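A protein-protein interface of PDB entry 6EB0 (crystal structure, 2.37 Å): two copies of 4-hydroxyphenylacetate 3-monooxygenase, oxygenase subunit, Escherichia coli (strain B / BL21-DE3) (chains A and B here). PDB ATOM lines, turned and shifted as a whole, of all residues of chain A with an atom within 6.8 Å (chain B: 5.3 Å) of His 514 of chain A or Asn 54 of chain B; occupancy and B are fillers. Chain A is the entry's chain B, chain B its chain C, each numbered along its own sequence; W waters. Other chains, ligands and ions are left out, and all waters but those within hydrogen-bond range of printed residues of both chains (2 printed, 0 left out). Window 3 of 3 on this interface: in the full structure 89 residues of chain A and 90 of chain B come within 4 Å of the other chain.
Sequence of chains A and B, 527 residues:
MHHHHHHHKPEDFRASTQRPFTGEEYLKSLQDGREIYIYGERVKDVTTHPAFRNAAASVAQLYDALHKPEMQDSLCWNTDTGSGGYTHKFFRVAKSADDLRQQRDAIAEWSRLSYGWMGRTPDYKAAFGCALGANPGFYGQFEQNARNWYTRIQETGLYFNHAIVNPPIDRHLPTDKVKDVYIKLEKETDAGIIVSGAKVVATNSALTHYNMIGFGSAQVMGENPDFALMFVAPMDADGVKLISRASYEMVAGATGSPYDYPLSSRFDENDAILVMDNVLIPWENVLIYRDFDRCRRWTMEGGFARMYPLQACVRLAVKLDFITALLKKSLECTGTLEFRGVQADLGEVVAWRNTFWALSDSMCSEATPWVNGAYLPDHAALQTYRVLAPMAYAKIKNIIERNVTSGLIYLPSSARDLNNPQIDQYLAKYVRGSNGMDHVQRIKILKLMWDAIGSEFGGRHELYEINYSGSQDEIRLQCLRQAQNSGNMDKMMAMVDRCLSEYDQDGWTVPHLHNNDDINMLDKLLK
OD2 of Asp 518 of chain A is in salt-bridge range of NH1 of Arg 53 of chain B (2.9 Å). N of His 514 of chain A lies within hydrogen-bond range of OD1 of Asn 54 of chain B, at 2.8 Å. The backbone carbonyl oxygen (O) of Asn 515 of chain A lies within hydrogen-bond range of the guanidinium group (NH2) of Arg 53 of chain B (3.2 Å).
The side-chain carboxylate of Glu 249 of chain B lies within hydrogen-bond range of the backbone NH of Arg 53 of chain B (3.2 Å). ND2 of Asn 54 of chain B is in hydrogen-bond range of O of Ser 265 of chain B (3.0 Å). O of Asn 54 of chain B is in hydrogen-bond range of OG of Ser 58 of chain B (3.1 Å). The backbone carbonyl oxygen of Arg 266 of chain B sits at hydrogen-bond distance from the side-chain hydroxyl of Ser 58 of chain B. The backbone NH of Asn 54 of chain B is in hydrogen-bond range of the side-chain carboxylate of Glu 249 of chain B, 2.7 Å away. The backbone carbonyl oxygen (O) of His 514 of chain A sits at hydrogen-bond distance from the indole nitrogen (NE1) of Trp 508 of chain A (2.9 Å).
Trp 508 of chain A touches Asn 54 of chain B. CZ2 of Trp 508 of chain A touches CB of Ser 265 of chain B (3.7 Å). Arg 266 of chain B touches Trp 508 of chain A (NE to CZ3, 3.5 Å). Ala 57 of chain B touches His 512 of chain A (CB to O, 3.4 Å). Asn 54 of chain B touches Leu 513 of chain A. CD1 of Leu 513 of chain A touches CD of Arg 266 of chain B (3.9 Å). Arg 53 of chain B touches His 514 of chain A (NE to CB, 3.5 Å).
Of the printed residues of chain B, Trp 508 of chain A touches Asn 54 (3.8 Å), Ser 265 (3.7 Å) and Arg 266 (3.5 Å). Of chain B, only Arg 53 and Asn 54 come within 4 Å of His 514 of chain A. Asn 54 of chain B touches just these residues of chain A: Trp 508 (3.8 Å), Leu 513 (3.7 Å) and His 514 (2.8 Å). Ala 56 of chain B touches none of the printed residues of chain A. Of the printed residues of chain A, Ser 265 of chain B touches Trp 508. Of the printed residues of chain A, Arg 266 of chain B touches Trp 508 and Leu 513. The nearest residue of chain A that does not touch Asn 54 of chain B is His 512 of chain A (4.9 Å). The nearest printed residue of chain A that does not touch Arg 266 of chain B is Val 510 of chain A (5.9 Å).
Of the 10 printed residues of chain A, 6 touch a printed residue of chain B. Along chain A the printed residues that touch a printed residue of chain B span positions 508 to 518. Along chain B the printed residues that touch a printed residue of chain A span positions 53 to 266.
No position is printed for both chains.
Water W1 lies within hydrogen-bond range of NE2 of His 512 of chain A and OG of Ser 58 of chain B. Water W2 bridges NH2 of Arg 53 of chain B (2.9 Å) and O of His 514 of chain A (3.0 Å).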
ATOM      1  N   TRP A 508      24.980 -13.159 -13.417  1.00  0.00           N
ATOM      2  CA  TRP A 508      24.248 -12.127 -12.716  1.00  0.00           C
ATOM      3  C   TRP A 508      22.756 -12.383 -12.845  1.00  0.00           C
ATOM      4  O   TRP A 508      22.285 -12.938 -13.832  1.00  0.00           O
ATOM      5  CB  TRP A 508      24.594 -10.744 -13.271  1.00  0.00           C
ATOM      6  CG  TRP A 508      26.048 -10.373 -13.216  1.00  0.00           C
ATOM      7  CD1 TRP A 508      26.882 -10.202 -14.272  1.00  0.00           C
ATOM      8  CD2 TRP A 508      26.841 -10.138 -12.039  1.00  0.00           C
ATOM      9  NE1 TRP A 508      28.146  -9.862 -13.834  1.00  0.00           N
ATOM     10  CE2 TRP A 508      28.145  -9.816 -12.469  1.00  0.00           C
ATOM     11  CE3 TRP A 508      26.574 -10.169 -10.672  1.00  0.00           C
ATOM     12  CZ2 TRP A 508      29.175  -9.515 -11.585  1.00  0.00           C
ATOM     13  CZ3 TRP A 508      27.604  -9.880  -9.786  1.00  0.00           C
ATOM     14  CH2 TRP A 508      28.895  -9.554 -10.250  1.00  0.00           C
ATOM     15  N   VAL A 510      20.893  -9.572 -12.107  1.00  0.00           N
ATOM     16  CA  VAL A 510      20.444  -8.192 -12.271  1.00  0.00           C
ATOM     17  C   VAL A 510      20.885  -7.705 -13.644  1.00  0.00           C
ATOM     18  O   VAL A 510      21.953  -8.103 -14.125  1.00  0.00           O
ATOM     19  CB  VAL A 510      20.973  -7.288 -11.147  1.00  0.00           C
ATOM     20  CG1 VAL A 510      20.319  -7.652  -9.827  1.00  0.00           C
ATOM     21  CG2 VAL A 510      22.476  -7.361 -11.053  1.00  0.00           C
ATOM     22  N   PRO A 511      20.119  -6.822 -14.290  1.00  0.00           N
ATOM     23  CA  PRO A 511      20.400  -6.495 -15.693  1.00  0.00           C
ATOM     24  C   PRO A 511      21.574  -5.558 -15.946  1.00  0.00           C
ATOM     25  O   PRO A 511      22.074  -5.549 -17.071  1.00  0.00           O
ATOM     26  CB  PRO A 511      19.080  -5.860 -16.172  1.00  0.00           C
ATOM     27  CG  PRO A 511      18.407  -5.391 -14.942  1.00  0.00           C
ATOM     28  CD  PRO A 511      18.819  -6.290 -13.842  1.00  0.00           C
ATOM     29  N   HIS A 512      22.045  -4.780 -14.979  1.00  0.00           N
ATOM     30  CA  HIS A 512      23.025  -3.757 -15.332  1.00  0.00           C
ATOM     31  C   HIS A 512      24.464  -4.265 -15.413  1.00  0.00           C
ATOM     32  O   HIS A 512      25.325  -3.525 -15.877  1.00  0.00           O
ATOM     33  CB  HIS A 512      22.959  -2.589 -14.346  1.00  0.00           C
ATOM     34  CG  HIS A 512      23.513  -2.910 -12.994  1.00  0.00           C
ATOM     35  ND1 HIS A 512      22.805  -3.621 -12.049  1.00  0.00           N
ATOM     36  CD2 HIS A 512      24.711  -2.625 -12.429  1.00  0.00           C
ATOM     37  CE1 HIS A 512      23.536  -3.748 -10.959  1.00  0.00           C
ATOM     38  NE2 HIS A 512      24.691  -3.146 -11.160  1.00  0.00           N
ATOM     39  N   LEU A 513      24.753  -5.489 -15.001  1.00  0.00           N
ATOM     40  CA  LEU A 513      26.110  -6.013 -15.031  1.00  0.00           C
ATOM     41  C   LEU A 513      26.324  -6.942 -16.224  1.00  0.00           C
ATOM     42  O   LEU A 513      25.392  -7.570 -16.729  1.00  0.00           O
ATOM     43  CB  LEU A 513      26.421  -6.743 -13.724  1.00  0.00           C
ATOM     44  CG  LEU A 513      26.417  -5.854 -12.477  1.00  0.00           C
ATOM     45  CD1 LEU A 513      26.503  -6.699 -11.225  1.00  0.00           C
ATOM     46  CD2 LEU A 513      27.574  -4.835 -12.501  1.00  0.00           C
ATOM     47  N   HIS A 514      27.563  -7.008 -16.684  1.00  0.00           N
ATOM     48  CA  HIS A 514      27.929  -7.825 -17.834  1.00  0.00           C
ATOM     49  C   HIS A 514      28.313  -9.225 -17.382  1.00  0.00           C
ATOM     50  O   HIS A 514      29.193  -9.383 -16.540  1.00  0.00           O
ATOM     51  CB  HIS A 514      29.092  -7.194 -18.597  1.00  0.00           C
ATOM     52  CG  HIS A 514      28.799  -5.825 -19.123  1.00  0.00           C
ATOM     53  ND1 HIS A 514      28.858  -4.695 -18.339  1.00  0.00           N
ATOM     54  CD2 HIS A 514      28.428  -5.408 -20.356  1.00  0.00           C
ATOM     55  CE1 HIS A 514      28.545  -3.639 -19.069  1.00  0.00           C
ATOM     56  NE2 HIS A 514      28.282  -4.045 -20.297  1.00  0.00           N
ATOM     57  N   ASN A 515      27.643 -10.237 -17.930  1.00  0.00           N
ATOM     58  CA  ASN A 515      28.118 -11.596 -17.731  1.00  0.00           C
ATOM     59  C   ASN A 515      29.422 -11.800 -18.492  1.00  0.00           C
ATOM     60  O   ASN A 515      29.761 -11.046 -19.400  1.00  0.00           O
ATOM     61  CB  ASN A 515      27.056 -12.613 -18.134  1.00  0.00           C
ATOM     62  CG  ASN A 515      25.933 -12.687 -17.120  1.00  0.00           C
ATOM     63  OD1 ASN A 515      26.154 -13.065 -15.963  1.00  0.00           O
ATOM     64  ND2 ASN A 515      24.724 -12.319 -17.535  1.00  0.00           N
ATOM     65  N   ASN A 516      30.176 -12.811 -18.083  1.00  0.00           N
ATOM     66  CA  ASN A 516      31.527 -12.999 -18.582  1.00  0.00           C
ATOM     67  C   ASN A 516      31.623 -14.105 -19.625  1.00  0.00           C
ATOM     68  O   ASN A 516      32.730 -14.534 -19.960  1.00  0.00           O
ATOM     69  CB  ASN A 516      32.475 -13.278 -17.410  1.00  0.00           C
ATOM     70  CG  ASN A 516      32.258 -14.653 -16.786  1.00  0.00           C
ATOM     71  OD1 ASN A 516      31.148 -15.158 -16.758  1.00  0.00           O
ATOM     72  ND2 ASN A 516      33.321 -15.251 -16.276  1.00  0.00           N
ATOM     73  N   ASP A 517      30.497 -14.562 -20.169  1.00  0.00           N
ATOM     74  CA  ASP A 517      30.573 -15.617 -21.169  1.00  0.00           C
ATOM     75  C   ASP A 517      31.311 -15.167 -22.421  1.00  0.00           C
ATOM     76  O   ASP A 517      31.880 -16.003 -23.126  1.00  0.00           O
ATOM     77  CB  ASP A 517      29.173 -16.133 -21.511  1.00  0.00           C
ATOM     78  CG  ASP A 517      28.132 -15.038 -21.554  1.00  0.00           C
ATOM     79  OD1 ASP A 517      28.435 -13.923 -22.035  1.00  0.00           O
ATOM     80  OD2 ASP A 517      27.004 -15.296 -21.087  1.00  0.00           O
ATOM     81  N   ASP A 518      31.346 -13.868 -22.697  1.00  0.00           N
ATOM     82  CA  ASP A 518      32.102 -13.362 -23.828  1.00  0.00           C
ATOM     83  C   ASP A 518      33.601 -13.236 -23.557  1.00  0.00           C
ATOM     84  O   ASP A 518      34.366 -13.104 -24.511  1.00  0.00           O
ATOM     85  CB  ASP A 518      31.535 -12.005 -24.252  1.00  0.00           C
ATOM     86  CG  ASP A 518      31.566 -10.973 -23.123  1.00  0.00           C
ATOM     87  OD1 ASP A 518      31.680 -11.363 -21.951  1.00  0.00           O
ATOM     88  OD2 ASP A 518      31.499  -9.762 -23.410  1.00  0.00           O
ATOM     89  N   THR B  47      33.599   1.873 -21.031  1.00  0.00           N
ATOM     90  CA  THR B  47      32.288   1.317 -20.720  1.00  0.00           C
ATOM     91  C   THR B  47      32.088  -0.070 -21.306  1.00  0.00           C
ATOM     92  O   THR B  47      31.152  -0.755 -20.898  1.00  0.00           O
ATOM     93  CB  THR B  47      31.143   2.220 -21.219  1.00  0.00           C
ATOM     94  OG1 THR B  47      31.144   2.278 -22.649  1.00  0.00           O
ATOM     95  CG2 THR B  47      31.250   3.629 -20.637  1.00  0.00           C
ATOM     96  N   PHE B  52      36.961  -2.765 -17.084  1.00  0.00           N
ATOM     97  CA  PHE B  52      36.313  -1.599 -16.502  1.00  0.00           C
ATOM     98  C   PHE B  52      34.803  -1.595 -16.603  1.00  0.00           C
ATOM     99  O   PHE B  52      34.167  -0.825 -15.890  1.00  0.00           O
ATOM    100  CB  PHE B  52      36.831  -0.317 -17.173  1.00  0.00           C
ATOM    101  CG  PHE B  52      38.311  -0.138 -17.087  1.00  0.00           C
ATOM    102  CD1 PHE B  52      38.894   0.419 -15.963  1.00  0.00           C
ATOM    103  CD2 PHE B  52      39.121  -0.512 -18.138  1.00  0.00           C
ATOM    104  CE1 PHE B  52      40.260   0.591 -15.891  1.00  0.00           C
ATOM    105  CE2 PHE B  52      40.490  -0.345 -18.074  1.00  0.00           C
ATOM    106  CZ  PHE B  52      41.063   0.206 -16.951  1.00  0.00           C
ATOM    107  N   ARG B  53      34.206  -2.415 -17.455  1.00  0.00           N
ATOM    108  CA  ARG B  53      32.810  -2.193 -17.811  1.00  0.00           C
ATOM    109  C   ARG B  53      31.873  -2.375 -16.613  1.00  0.00           C
ATOM    110  O   ARG B  53      30.908  -1.619 -16.460  1.00  0.00           O
ATOM    111  CB  ARG B  53      32.431  -3.114 -18.971  1.00  0.00           C
ATOM    112  CG  ARG B  53      32.599  -4.581 -18.643  1.00  0.00           C
ATOM    113  CD  ARG B  53      32.465  -5.441 -19.884  1.00  0.00           C
ATOM    114  NE  ARG B  53      32.495  -6.851 -19.536  1.00  0.00           N
ATOM    115  CZ  ARG B  53      32.239  -7.839 -20.381  1.00  0.00           C
ATOM    116  NH1 ARG B  53      31.927  -7.571 -21.631  1.00  0.00           N
ATOM    117  NH2 ARG B  53      32.288  -9.088 -19.964  1.00  0.00           N
ATOM    118  N   ASN B  54      32.139  -3.356 -15.747  1.00  0.00           N
ATOM    119  CA  ASN B  54      31.234  -3.558 -14.615  1.00  0.00           C
ATOM    120  C   ASN B  54      31.449  -2.524 -13.519  1.00  0.00           C
ATOM    121  O   ASN B  54      30.477  -2.039 -12.938  1.00  0.00           O
ATOM    122  CB  ASN B  54      31.352  -4.976 -14.050  1.00  0.00           C
ATOM    123  CG  ASN B  54      30.591  -5.988 -14.892  1.00  0.00           C
ATOM    124  OD1 ASN B  54      29.769  -5.603 -15.711  1.00  0.00           O
ATOM    125  ND2 ASN B  54      30.857  -7.275 -14.694  1.00  0.00           N
ATOM    126  N   ALA B  55      32.706  -2.161 -13.242  1.00  0.00           N
ATOM    127  CA  ALA B  55      32.972  -1.066 -12.318  1.00  0.00           C
ATOM    128  C   ALA B  55      32.292   0.211 -12.789  1.00  0.00           C
ATOM    129  O   ALA B  55      31.776   0.981 -11.976  1.00  0.00           O
ATOM    130  CB  ALA B  55      34.478  -0.841 -12.173  1.00  0.00           C
ATOM    131  N   ALA B  56      32.304   0.454 -14.104  1.00  0.00           N
ATOM    132  CA  ALA B  56      31.602   1.608 -14.639  1.00  0.00           C
ATOM    133  C   ALA B  56      30.102   1.465 -14.454  1.00  0.00           C
ATOM    134  O   ALA B  56      29.428   2.435 -14.109  1.00  0.00           O
ATOM    135  CB  ALA B  56      31.943   1.809 -16.117  1.00  0.00           C
ATOM    136  N   ALA B  57      29.569   0.258 -14.671  1.00  0.00           N
ATOM    137  CA  ALA B  57      28.140   0.022 -14.479  1.00  0.00           C
ATOM    138  C   ALA B  57      27.739   0.231 -13.018  1.00  0.00           C
ATOM    139  O   ALA B  57      26.663   0.757 -12.736  1.00  0.00           O
ATOM    140  CB  ALA B  57      27.771  -1.382 -14.962  1.00  0.00           C
ATOM    141  N   SER B  58      28.613  -0.150 -12.085  1.00  0.00           N
ATOM    142  CA  SER B  58      28.352   0.031 -10.661  1.00  0.00           C
ATOM    143  C   SER B  58      28.284   1.508 -10.284  1.00  0.00           C
ATOM    144  O   SER B  58      27.422   1.912  -9.501  1.00  0.00           O
ATOM    145  CB  SER B  58      29.437  -0.664  -9.840  1.00  0.00           C
ATOM    146  OG  SER B  58      29.430  -2.050 -10.030  1.00  0.00           O
ATOM    147  N   VAL B  59      29.185   2.329 -10.824  1.00  0.00           N
ATOM    148  CA  VAL B  59      29.099   3.765 -10.582  1.00  0.00           C
ATOM    149  C   VAL B  59      27.832   4.346 -11.207  1.00  0.00           C
ATOM    150  O   VAL B  59      27.190   5.223 -10.624  1.00  0.00           O
ATOM    151  CB  VAL B  59      30.368   4.484 -11.078  1.00  0.00           C
ATOM    152  CG1 VAL B  59      30.201   5.992 -10.962  1.00  0.00           C
ATOM    153  CG2 VAL B  59      31.561   4.068 -10.249  1.00  0.00           C
ATOM    154  N   GLU B 249      38.820  -7.144 -11.964  1.00  0.00           N
ATOM    155  CA  GLU B 249      37.598  -7.372 -12.731  1.00  0.00           C
ATOM    156  C   GLU B 249      37.881  -8.237 -13.960  1.00  0.00           C
ATOM    157  O   GLU B 249      37.210  -9.248 -14.190  1.00  0.00           O
ATOM    158  CB  GLU B 249      36.963  -6.031 -13.136  1.00  0.00           C
ATOM    159  CG  GLU B 249      35.844  -6.184 -14.160  1.00  0.00           C
ATOM    160  CD  GLU B 249      35.025  -4.921 -14.488  1.00  0.00           C
ATOM    161  OE1 GLU B 249      35.097  -3.898 -13.792  1.00  0.00           O
ATOM    162  OE2 GLU B 249      34.290  -4.959 -15.484  1.00  0.00           O
ATOM    163  N   SER B 265      34.342  -8.884  -9.523  1.00  0.00           N
ATOM    164  CA  SER B 265      33.735  -8.813 -10.841  1.00  0.00           C
ATOM    165  C   SER B 265      32.974  -7.522 -11.080  1.00  0.00           C
ATOM    166  O   SER B 265      32.616  -7.252 -12.227  1.00  0.00           O
ATOM    167  CB  SER B 265      32.784  -9.985 -11.060  1.00  0.00           C
ATOM    168  OG  SER B 265      33.466 -11.214 -11.040  1.00  0.00           O
ATOM    169  N   ARG B 266      32.731  -6.711 -10.050  1.00  0.00           N
ATOM    170  CA  ARG B 266      31.907  -5.523 -10.259  1.00  0.00           C
ATOM    171  C   ARG B 266      32.334  -4.271  -9.502  1.00  0.00           C
ATOM    172  O   ARG B 266      31.869  -3.197  -9.868  1.00  0.00           O
ATOM    173  CB  ARG B 266      30.445  -5.837  -9.904  1.00  0.00           C
ATOM    174  CG  ARG B 266      30.245  -6.239  -8.485  1.00  0.00           C
ATOM    175  CD  ARG B 266      28.783  -6.390  -8.133  1.00  0.00           C
ATOM    176  NE  ARG B 266      28.607  -7.583  -7.306  1.00  0.00           N
ATOM    177  CZ  ARG B 266      27.499  -7.900  -6.649  1.00  0.00           C
ATOM    178  NH1 ARG B 266      26.441  -7.104  -6.703  1.00  0.00           N
ATOM    179  NH2 ARG B 266      27.460  -9.017  -5.939  1.00  0.00           N
HETATM  180  O   HOH W   1      26.559  -2.760  -9.045  1.00  0.00           O
HETATM  181  O   HOH W   2      32.135  -9.725 -17.118  1.00  0.00           O
